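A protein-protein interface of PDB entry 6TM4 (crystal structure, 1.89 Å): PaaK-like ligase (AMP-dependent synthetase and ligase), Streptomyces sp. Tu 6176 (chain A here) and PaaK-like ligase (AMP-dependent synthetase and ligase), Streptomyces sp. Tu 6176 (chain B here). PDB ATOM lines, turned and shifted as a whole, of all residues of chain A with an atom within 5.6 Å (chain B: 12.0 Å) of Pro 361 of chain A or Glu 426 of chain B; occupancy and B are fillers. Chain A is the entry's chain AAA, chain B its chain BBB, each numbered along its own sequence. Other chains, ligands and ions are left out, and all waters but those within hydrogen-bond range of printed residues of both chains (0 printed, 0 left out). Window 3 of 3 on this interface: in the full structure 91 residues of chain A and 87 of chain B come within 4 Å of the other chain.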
ATOM      1  N   ARG A 328      18.462  -5.242 -20.183  1.00  0.00           N
ATOM      2  CA  ARG A 328      18.716  -3.778 -20.188  1.00  0.00           C
ATOM      3  C   ARG A 328      19.357  -3.403 -21.527  1.00  0.00           C
ATOM      4  O   ARG A 328      20.317  -4.080 -21.940  1.00  0.00           O
ATOM      5  CB  ARG A 328      19.607  -3.365 -19.014  1.00  0.00           C
ATOM      6  CG  ARG A 328      18.955  -3.534 -17.649  1.00  0.00           C
ATOM      7  CD  ARG A 328      17.981  -2.418 -17.297  1.00  0.00           C
ATOM      8  NE  ARG A 328      17.342  -2.648 -16.001  1.00  0.00           N
ATOM      9  CZ  ARG A 328      17.907  -2.437 -14.809  1.00  0.00           C
ATOM     10  NH1 ARG A 328      19.144  -1.972 -14.718  1.00  0.00           N
ATOM     11  NH2 ARG A 328      17.231  -2.697 -13.701  1.00  0.00           N
ATOM     12  N   ILE A 329      18.814  -2.375 -22.178  1.00  0.00           N
ATOM     13  CA  ILE A 329      19.277  -1.857 -23.502  1.00  0.00           C
ATOM     14  C   ILE A 329      19.323  -0.334 -23.386  1.00  0.00           C
ATOM     15  O   ILE A 329      18.268   0.304 -23.586  1.00  0.00           O
ATOM     16  CB  ILE A 329      18.348  -2.321 -24.647  1.00  0.00           C
ATOM     17  CG1 ILE A 329      18.113  -3.835 -24.613  1.00  0.00           C
ATOM     18  CG2 ILE A 329      18.876  -1.843 -25.995  1.00  0.00           C
ATOM     19  CD1 ILE A 329      17.400  -4.371 -25.816  1.00  0.00           C
ATOM     20  N   GLY A 330      20.502   0.209 -23.057  1.00  0.00           N
ATOM     21  CA  GLY A 330      20.674   1.592 -22.579  1.00  0.00           C
ATOM     22  C   GLY A 330      19.736   1.878 -21.408  1.00  0.00           C
ATOM     23  O   GLY A 330      19.732   1.138 -20.420  1.00  0.00           O
ATOM     24  N   LYS A 358      17.169  -9.837 -30.432  1.00  0.00           N
ATOM     25  CA  LYS A 358      18.343 -10.002 -29.549  1.00  0.00           C
ATOM     26  C   LYS A 358      18.578  -8.680 -28.816  1.00  0.00           C
ATOM     27  O   LYS A 358      18.644  -7.626 -29.520  1.00  0.00           O
ATOM     28  CB  LYS A 358      19.560 -10.419 -30.372  1.00  0.00           C
ATOM     29  CG  LYS A 358      20.732 -10.935 -29.547  1.00  0.00           C
ATOM     30  CD  LYS A 358      21.901 -11.375 -30.383  1.00  0.00           C
ATOM     31  CE  LYS A 358      21.669 -12.669 -31.126  1.00  0.00           C
ATOM     32  NZ  LYS A 358      22.433 -12.672 -32.395  1.00  0.00           N
ATOM     33  N   ALA A 359      18.670  -8.757 -27.479  1.00  0.00           N
ATOM     34  CA  ALA A 359      19.125  -7.669 -26.588  1.00  0.00           C
ATOM     35  C   ALA A 359      20.657  -7.565 -26.637  1.00  0.00           C
ATOM     36  O   ALA A 359      21.327  -8.457 -26.084  1.00  0.00           O
ATOM     37  CB  ALA A 359      18.634  -7.904 -25.181  1.00  0.00           C
ATOM     38  N   HIS A 360      21.191  -6.534 -27.294  1.00  0.00           N
ATOM     39  CA  HIS A 360      22.598  -6.105 -27.131  1.00  0.00           C
ATOM     40  C   HIS A 360      22.603  -5.041 -26.037  1.00  0.00           C
ATOM     41  O   HIS A 360      21.552  -4.469 -25.725  1.00  0.00           O
ATOM     42  CB  HIS A 360      23.191  -5.608 -28.456  1.00  0.00           C
ATOM     43  CG  HIS A 360      23.056  -6.566 -29.593  1.00  0.00           C
ATOM     44  ND1 HIS A 360      23.995  -7.548 -29.852  1.00  0.00           N
ATOM     45  CD2 HIS A 360      22.118  -6.678 -30.561  1.00  0.00           C
ATOM     46  CE1 HIS A 360      23.642  -8.227 -30.928  1.00  0.00           C
ATOM     47  NE2 HIS A 360      22.490  -7.707 -31.386  1.00  0.00           N
ATOM     48  N   PRO A 361      23.766  -4.764 -25.400  1.00  0.00           N
ATOM     49  CA  PRO A 361      23.853  -3.715 -24.386  1.00  0.00           C
ATOM     50  C   PRO A 361      23.343  -2.261 -24.822  1.00  0.00           C
ATOM     51  O   PRO A 361      23.077  -1.461 -24.025  1.00  0.00           O
ATOM     52  CB  PRO A 361      25.368  -3.601 -24.095  1.00  0.00           C
ATOM     53  CG  PRO A 361      25.936  -4.961 -24.485  1.00  0.00           C
ATOM     54  CD  PRO A 361      25.037  -5.479 -25.593  1.00  0.00           C
ATOM     55  N   ASP A 362      23.495  -2.006 -26.151  1.00  0.00           N
ATOM     56  CA  ASP A 362      23.246  -0.669 -26.766  1.00  0.00           C
ATOM     57  C   ASP A 362      22.006  -0.654 -27.678  1.00  0.00           C
ATOM     58  O   ASP A 362      21.513   0.454 -27.920  1.00  0.00           O
ATOM     59  CB  ASP A 362      24.468  -0.187 -27.564  1.00  0.00           C
ATOM     60  CG  ASP A 362      24.890  -1.089 -28.729  1.00  0.00           C
ATOM     61  OD1 ASP A 362      24.696  -2.525 -28.385  1.00  0.00           O
ATOM     62  OD2 ASP A 362      25.101  -0.525 -29.935  1.00  0.00           O
ATOM     63  N   VAL A 363      21.521  -1.797 -28.178  1.00  0.00           N
ATOM     64  CA  VAL A 363      20.530  -1.800 -29.293  1.00  0.00           C
ATOM     65  C   VAL A 363      19.684  -3.077 -29.242  1.00  0.00           C
ATOM     66  O   VAL A 363      20.209  -4.134 -28.850  1.00  0.00           O
ATOM     67  CB  VAL A 363      21.232  -1.584 -30.654  1.00  0.00           C
ATOM     68  CG1 VAL A 363      22.183  -2.715 -31.022  1.00  0.00           C
ATOM     69  CG2 VAL A 363      20.238  -1.336 -31.783  1.00  0.00           C
ATOM     70  N   ARG B 421      11.115 -19.223 -28.258  1.00  0.00           N
ATOM     71  CA  ARG B 421      11.565 -17.982 -27.586  1.00  0.00           C
ATOM     72  C   ARG B 421      11.727 -16.908 -28.661  1.00  0.00           C
ATOM     73  O   ARG B 421      12.132 -17.249 -29.800  1.00  0.00           O
ATOM     74  CB  ARG B 421      12.892 -18.190 -26.849  1.00  0.00           C
ATOM     75  CG  ARG B 421      12.846 -19.247 -25.755  1.00  0.00           C
ATOM     76  CD  ARG B 421      14.154 -19.280 -25.005  1.00  0.00           C
ATOM     77  NE  ARG B 421      14.461 -17.942 -24.521  1.00  0.00           N
ATOM     78  CZ  ARG B 421      15.682 -17.495 -24.299  1.00  0.00           C
ATOM     79  NH1 ARG B 421      16.728 -18.275 -24.499  1.00  0.00           N
ATOM     80  NH2 ARG B 421      15.859 -16.265 -23.856  1.00  0.00           N
ATOM     81  N   TYR B 422      11.376 -15.667 -28.298  1.00  0.00           N
ATOM     82  CA  TYR B 422      11.370 -14.562 -29.283  1.00  0.00           C
ATOM     83  C   TYR B 422      12.465 -13.522 -28.955  1.00  0.00           C
ATOM     84  O   TYR B 422      12.971 -12.834 -29.916  1.00  0.00           O
ATOM     85  CB  TYR B 422       9.949 -14.022 -29.396  1.00  0.00           C
ATOM     86  CG  TYR B 422       9.028 -15.030 -30.028  1.00  0.00           C
ATOM     87  CD1 TYR B 422       8.380 -16.002 -29.279  1.00  0.00           C
ATOM     88  CD2 TYR B 422       8.825 -15.019 -31.395  1.00  0.00           C
ATOM     89  CE1 TYR B 422       7.533 -16.919 -29.876  1.00  0.00           C
ATOM     90  CE2 TYR B 422       7.982 -15.929 -32.011  1.00  0.00           C
ATOM     91  CZ  TYR B 422       7.332 -16.893 -31.251  1.00  0.00           C
ATOM     92  OH  TYR B 422       6.525 -17.815 -31.877  1.00  0.00           O
ATOM     93  N   LEU B 423      12.775 -13.334 -27.672  1.00  0.00           N
ATOM     94  CA  LEU B 423      13.812 -12.357 -27.208  1.00  0.00           C
ATOM     95  C   LEU B 423      14.985 -13.141 -26.589  1.00  0.00           C
ATOM     96  O   LEU B 423      14.735 -14.049 -25.716  1.00  0.00           O
ATOM     97  CB  LEU B 423      13.188 -11.401 -26.195  1.00  0.00           C
ATOM     98  CG  LEU B 423      14.147 -10.421 -25.537  1.00  0.00           C
ATOM     99  CD1 LEU B 423      14.894  -9.583 -26.571  1.00  0.00           C
ATOM    100  CD2 LEU B 423      13.381  -9.496 -24.601  1.00  0.00           C
ATOM    101  N   PHE B 424      16.204 -12.820 -27.090  1.00  0.00           N
ATOM    102  CA  PHE B 424      17.453 -13.525 -26.700  1.00  0.00           C
ATOM    103  C   PHE B 424      18.420 -12.519 -26.086  1.00  0.00           C
ATOM    104  O   PHE B 424      18.352 -11.329 -26.475  1.00  0.00           O
ATOM    105  CB  PHE B 424      18.045 -14.223 -27.924  1.00  0.00           C
ATOM    106  CG  PHE B 424      17.219 -15.389 -28.373  1.00  0.00           C
ATOM    107  CD1 PHE B 424      16.109 -15.203 -29.185  1.00  0.00           C
ATOM    108  CD2 PHE B 424      17.503 -16.665 -27.921  1.00  0.00           C
ATOM    109  CE1 PHE B 424      15.327 -16.275 -29.571  1.00  0.00           C
ATOM    110  CE2 PHE B 424      16.720 -17.736 -28.303  1.00  0.00           C
ATOM    111  CZ  PHE B 424      15.632 -17.540 -29.127  1.00  0.00           C
ATOM    112  N   ALA B 425      19.279 -12.986 -25.172  1.00  0.00           N
ATOM    113  CA  ALA B 425      20.438 -12.220 -24.648  1.00  0.00           C
ATOM    114  C   ALA B 425      21.528 -12.206 -25.723  1.00  0.00           C
ATOM    115  O   ALA B 425      21.491 -13.067 -26.620  1.00  0.00           O
ATOM    116  CB  ALA B 425      20.939 -12.818 -23.355  1.00  0.00           C
ATOM    117  N   GLU B 426      22.481 -11.287 -25.632  1.00  0.00           N
ATOM    118  CA  GLU B 426      23.456 -11.031 -26.729  1.00  0.00           C
ATOM    119  C   GLU B 426      24.238 -12.296 -27.098  1.00  0.00           C
ATOM    120  O   GLU B 426      24.523 -12.493 -28.310  1.00  0.00           O
ATOM    121  CB  GLU B 426      24.436  -9.936 -26.342  1.00  0.00           C
ATOM    122  CG  GLU B 426      25.152  -9.400 -27.552  1.00  0.00           C
ATOM    123  CD  GLU B 426      26.368  -8.571 -27.236  1.00  0.00           C
ATOM    124  OE1 GLU B 426      26.597  -7.601 -27.964  1.00  0.00           O
ATOM    125  OE2 GLU B 426      27.074  -8.906 -26.265  1.00  0.00           O
ATOM    126  N   ASP B 427      24.540 -13.131 -26.105  1.00  0.00           N
ATOM    127  CA  ASP B 427      25.484 -14.272 -26.237  1.00  0.00           C
ATOM    128  C   ASP B 427      24.750 -15.561 -26.615  1.00  0.00           C
ATOM    129  O   ASP B 427      25.457 -16.551 -26.799  1.00  0.00           O
ATOM    130  CB  ASP B 427      26.296 -14.459 -24.952  1.00  0.00           C
ATOM    131  CG  ASP B 427      25.537 -14.064 -23.699  1.00  0.00           C
ATOM    132  OD1 ASP B 427      24.503 -14.710 -23.408  1.00  0.00           O
ATOM    133  OD2 ASP B 427      25.974 -13.089 -23.046  1.00  0.00           O
ATOM    134  N   GLU B 428      23.413 -15.545 -26.740  1.00  0.00           N
ATOM    135  CA  GLU B 428      22.611 -16.754 -27.077  1.00  0.00           C
ATOM    136  C   GLU B 428      22.501 -16.920 -28.602  1.00  0.00           C
ATOM    137  O   GLU B 428      22.526 -15.931 -29.338  1.00  0.00           O
ATOM    138  CB  GLU B 428      21.208 -16.698 -26.466  1.00  0.00           C
ATOM    139  CG  GLU B 428      21.166 -16.360 -24.983  1.00  0.00           C
ATOM    140  CD  GLU B 428      19.790 -16.542 -24.364  1.00  0.00           C
ATOM    141  OE1 GLU B 428      19.049 -15.559 -24.255  1.00  0.00           O
ATOM    142  OE2 GLU B 428      19.451 -17.688 -24.019  1.00  0.00           O
ATOM    143  N   ASP B 429      22.369 -18.163 -29.042  1.00  0.00           N
ATOM    144  CA  ASP B 429      22.023 -18.546 -30.433  1.00  0.00           C
ATOM    145  C   ASP B 429      20.521 -18.304 -30.642  1.00  0.00           C
ATOM    146  O   ASP B 429      19.734 -19.116 -30.107  1.00  0.00           O
ATOM    147  CB  ASP B 429      22.401 -20.016 -30.659  1.00  0.00           C
ATOM    148  CG  ASP B 429      22.072 -20.542 -32.043  1.00  0.00           C
ATOM    149  OD1 ASP B 429      22.166 -19.720 -32.987  1.00  0.00           O
ATOM    150  OD2 ASP B 429      21.668 -21.747 -32.157  1.00  0.00           O
ATOM    151  N   TRP B 430      20.124 -17.254 -31.383  1.00  0.00           N
ATOM    152  CA  TRP B 430      18.680 -16.985 -31.672  1.00  0.00           C
ATOM    153  C   TRP B 430      18.175 -17.844 -32.845  1.00  0.00           C
ATOM    154  O   TRP B 430      16.982 -17.704 -33.203  1.00  0.00           O
ATOM    155  CB  TRP B 430      18.369 -15.493 -31.881  1.00  0.00           C
ATOM    156  CG  TRP B 430      18.875 -14.864 -33.141  1.00  0.00           C
ATOM    157  CD1 TRP B 430      19.810 -15.356 -34.001  1.00  0.00           C
ATOM    158  CD2 TRP B 430      18.499 -13.576 -33.654  1.00  0.00           C
ATOM    159  NE1 TRP B 430      20.057 -14.455 -35.000  1.00  0.00           N
ATOM    160  CE2 TRP B 430      19.266 -13.353 -34.818  1.00  0.00           C
ATOM    161  CE3 TRP B 430      17.616 -12.576 -33.230  1.00  0.00           C
ATOM    162  CZ2 TRP B 430      19.166 -12.183 -35.571  1.00  0.00           C
ATOM    163  CZ3 TRP B 430      17.516 -11.420 -33.975  1.00  0.00           C
ATOM    164  CH2 TRP B 430      18.279 -11.226 -35.131  1.00  0.00           C
ATOM    165  N   ASP B 431      19.004 -18.741 -33.389  1.00  0.00           N
ATOM    166  CA  ASP B 431      18.582 -19.722 -34.425  1.00  0.00           C
ATOM    167  C   ASP B 431      17.438 -20.621 -33.906  1.00  0.00           C
ATOM    168  O   ASP B 431      16.728 -21.168 -34.750  1.00  0.00           O
ATOM    169  CB  ASP B 431      19.763 -20.567 -34.919  1.00  0.00           C
ATOM    170  CG  ASP B 431      19.454 -21.300 -36.211  1.00  0.00           C
ATOM    171  OD1 ASP B 431      19.510 -20.570 -37.308  1.00  0.00           O
ATOM    172  OD2 ASP B 431      19.117 -22.584 -36.108  1.00  0.00           O
ATOM    173  N   LYS B 432      17.255 -20.758 -32.585  1.00  0.00           N
ATOM    174  CA  LYS B 432      16.235 -21.662 -31.968  1.00  0.00           C
ATOM    175  C   LYS B 432      14.918 -20.911 -31.701  1.00  0.00           C
ATOM    176  O   LYS B 432      14.083 -21.453 -30.931  1.00  0.00           O
ATOM    177  CB  LYS B 432      16.777 -22.231 -30.649  1.00  0.00           C
ATOM    178  CG  LYS B 432      18.208 -22.764 -30.711  1.00  0.00           C
ATOM    179  CD  LYS B 432      18.357 -23.896 -31.704  1.00  0.00           C
ATOM    180  CE  LYS B 432      18.025 -25.237 -31.085  1.00  0.00           C
ATOM    181  NZ  LYS B 432      17.831 -26.297 -32.102  1.00  0.00           N
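N of Ala 359 of chain A sits at hydrogen-bond distance from O of Phe 424 of chain B (2.8 Å).
O of Ala 359 of chain A is in hydrogen-bond range of N of Glu 426 of chain B, at 3.1 Å.
A ring nitrogen (ND1) of His 360 of chain A sits close to the side-chain carboxylate (OE1) of Glu 426 of chain B.
Pro 361 of chain A touches one residue of chain B.
Of chain A, only Lys 358 (3.5 Å), Ala 359 (3.1 Å), His 360 (3.2 Å) and Pro 361 (3.5 Å) come within 4 Å of Glu 426 of chain B.
No residue of chain B comes within 4 Å of Ile 329 of chain A.
No residue of chain B comes within 4 Å of Gly 330 of chain A.
Lys 358 of chain A touches five residues of chain B.
Ala 359 of chain A touches just these residues of chain B: Leu 423, Phe 424, Ala 425 and Glu 426.
Printed residues of chain A within 4 Å of Trp 430 of chain B: Lys 358.
Of the printed residues of chain A, Leu 423 of chain B touches Ala 359.
Tyr 422 of chain B touches none of the printed residues of chain A.
Lys 432 of chain B touches none of the printed residues of chain A.
The nearest residue of chain B that does not touch Pro 361 of chain A is Ala 425 of chain B (7.6 Å).
The nearest printed residue of chain A that does not touch Trp 430 of chain B is His 360 of chain A (6.6 Å).
Hydrophobic or aromatic side chains of chain B within 4 Å of the printed part of chain A: Leu 423 and Trp 430.
Of the 9 printed residues of chain A, 4 touch a printed residue of chain B.
The backbone NH (N) of Gly 330 of chain A lies within hydrogen-bond range of the backbone carbonyl oxygen (O) of Pro 361 of chain A (3.2 Å).
The guanidinium group (NH2) of Arg 421 of chain B lies within hydrogen-bond range of the backbone carbonyl oxygen (O) of Leu 423 of chain B (3.1 Å).
The side-chain carboxylate (OE2) of Glu 428 of chain B lies within salt-bridge range of the guanidinium group (NH1) of Arg 421 of chain B (2.8 Å).
The backbone NH of Ala 425 of chain B sits at hydrogen-bond distance from the side-chain carboxylate of Glu 428 of chain B, 2.7 Å away.
Among the printed residues, pairs that only touch across the chains: Lys 358 of chain A with Phe 424 of chain B (3.3 Å), Lys 358 of chain A with Glu 426 of chain B (3.5 Å), Pro 361 of chain A with Glu 426 of chain B (3.5 Å), Lys 358 of chain A with Ala 425 of chain B (3.7 Å), Ala 359 of chain A with Ala 425 of chain B (3.8 Å), Lys 358 of chain A with Glu 428 of chain B (3.8 Å), Lys 358 of chain A with Trp 430 of chain B (3.9 Å) and Ala 359 of chain A with Leu 423 of chain B (3.97 Å).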
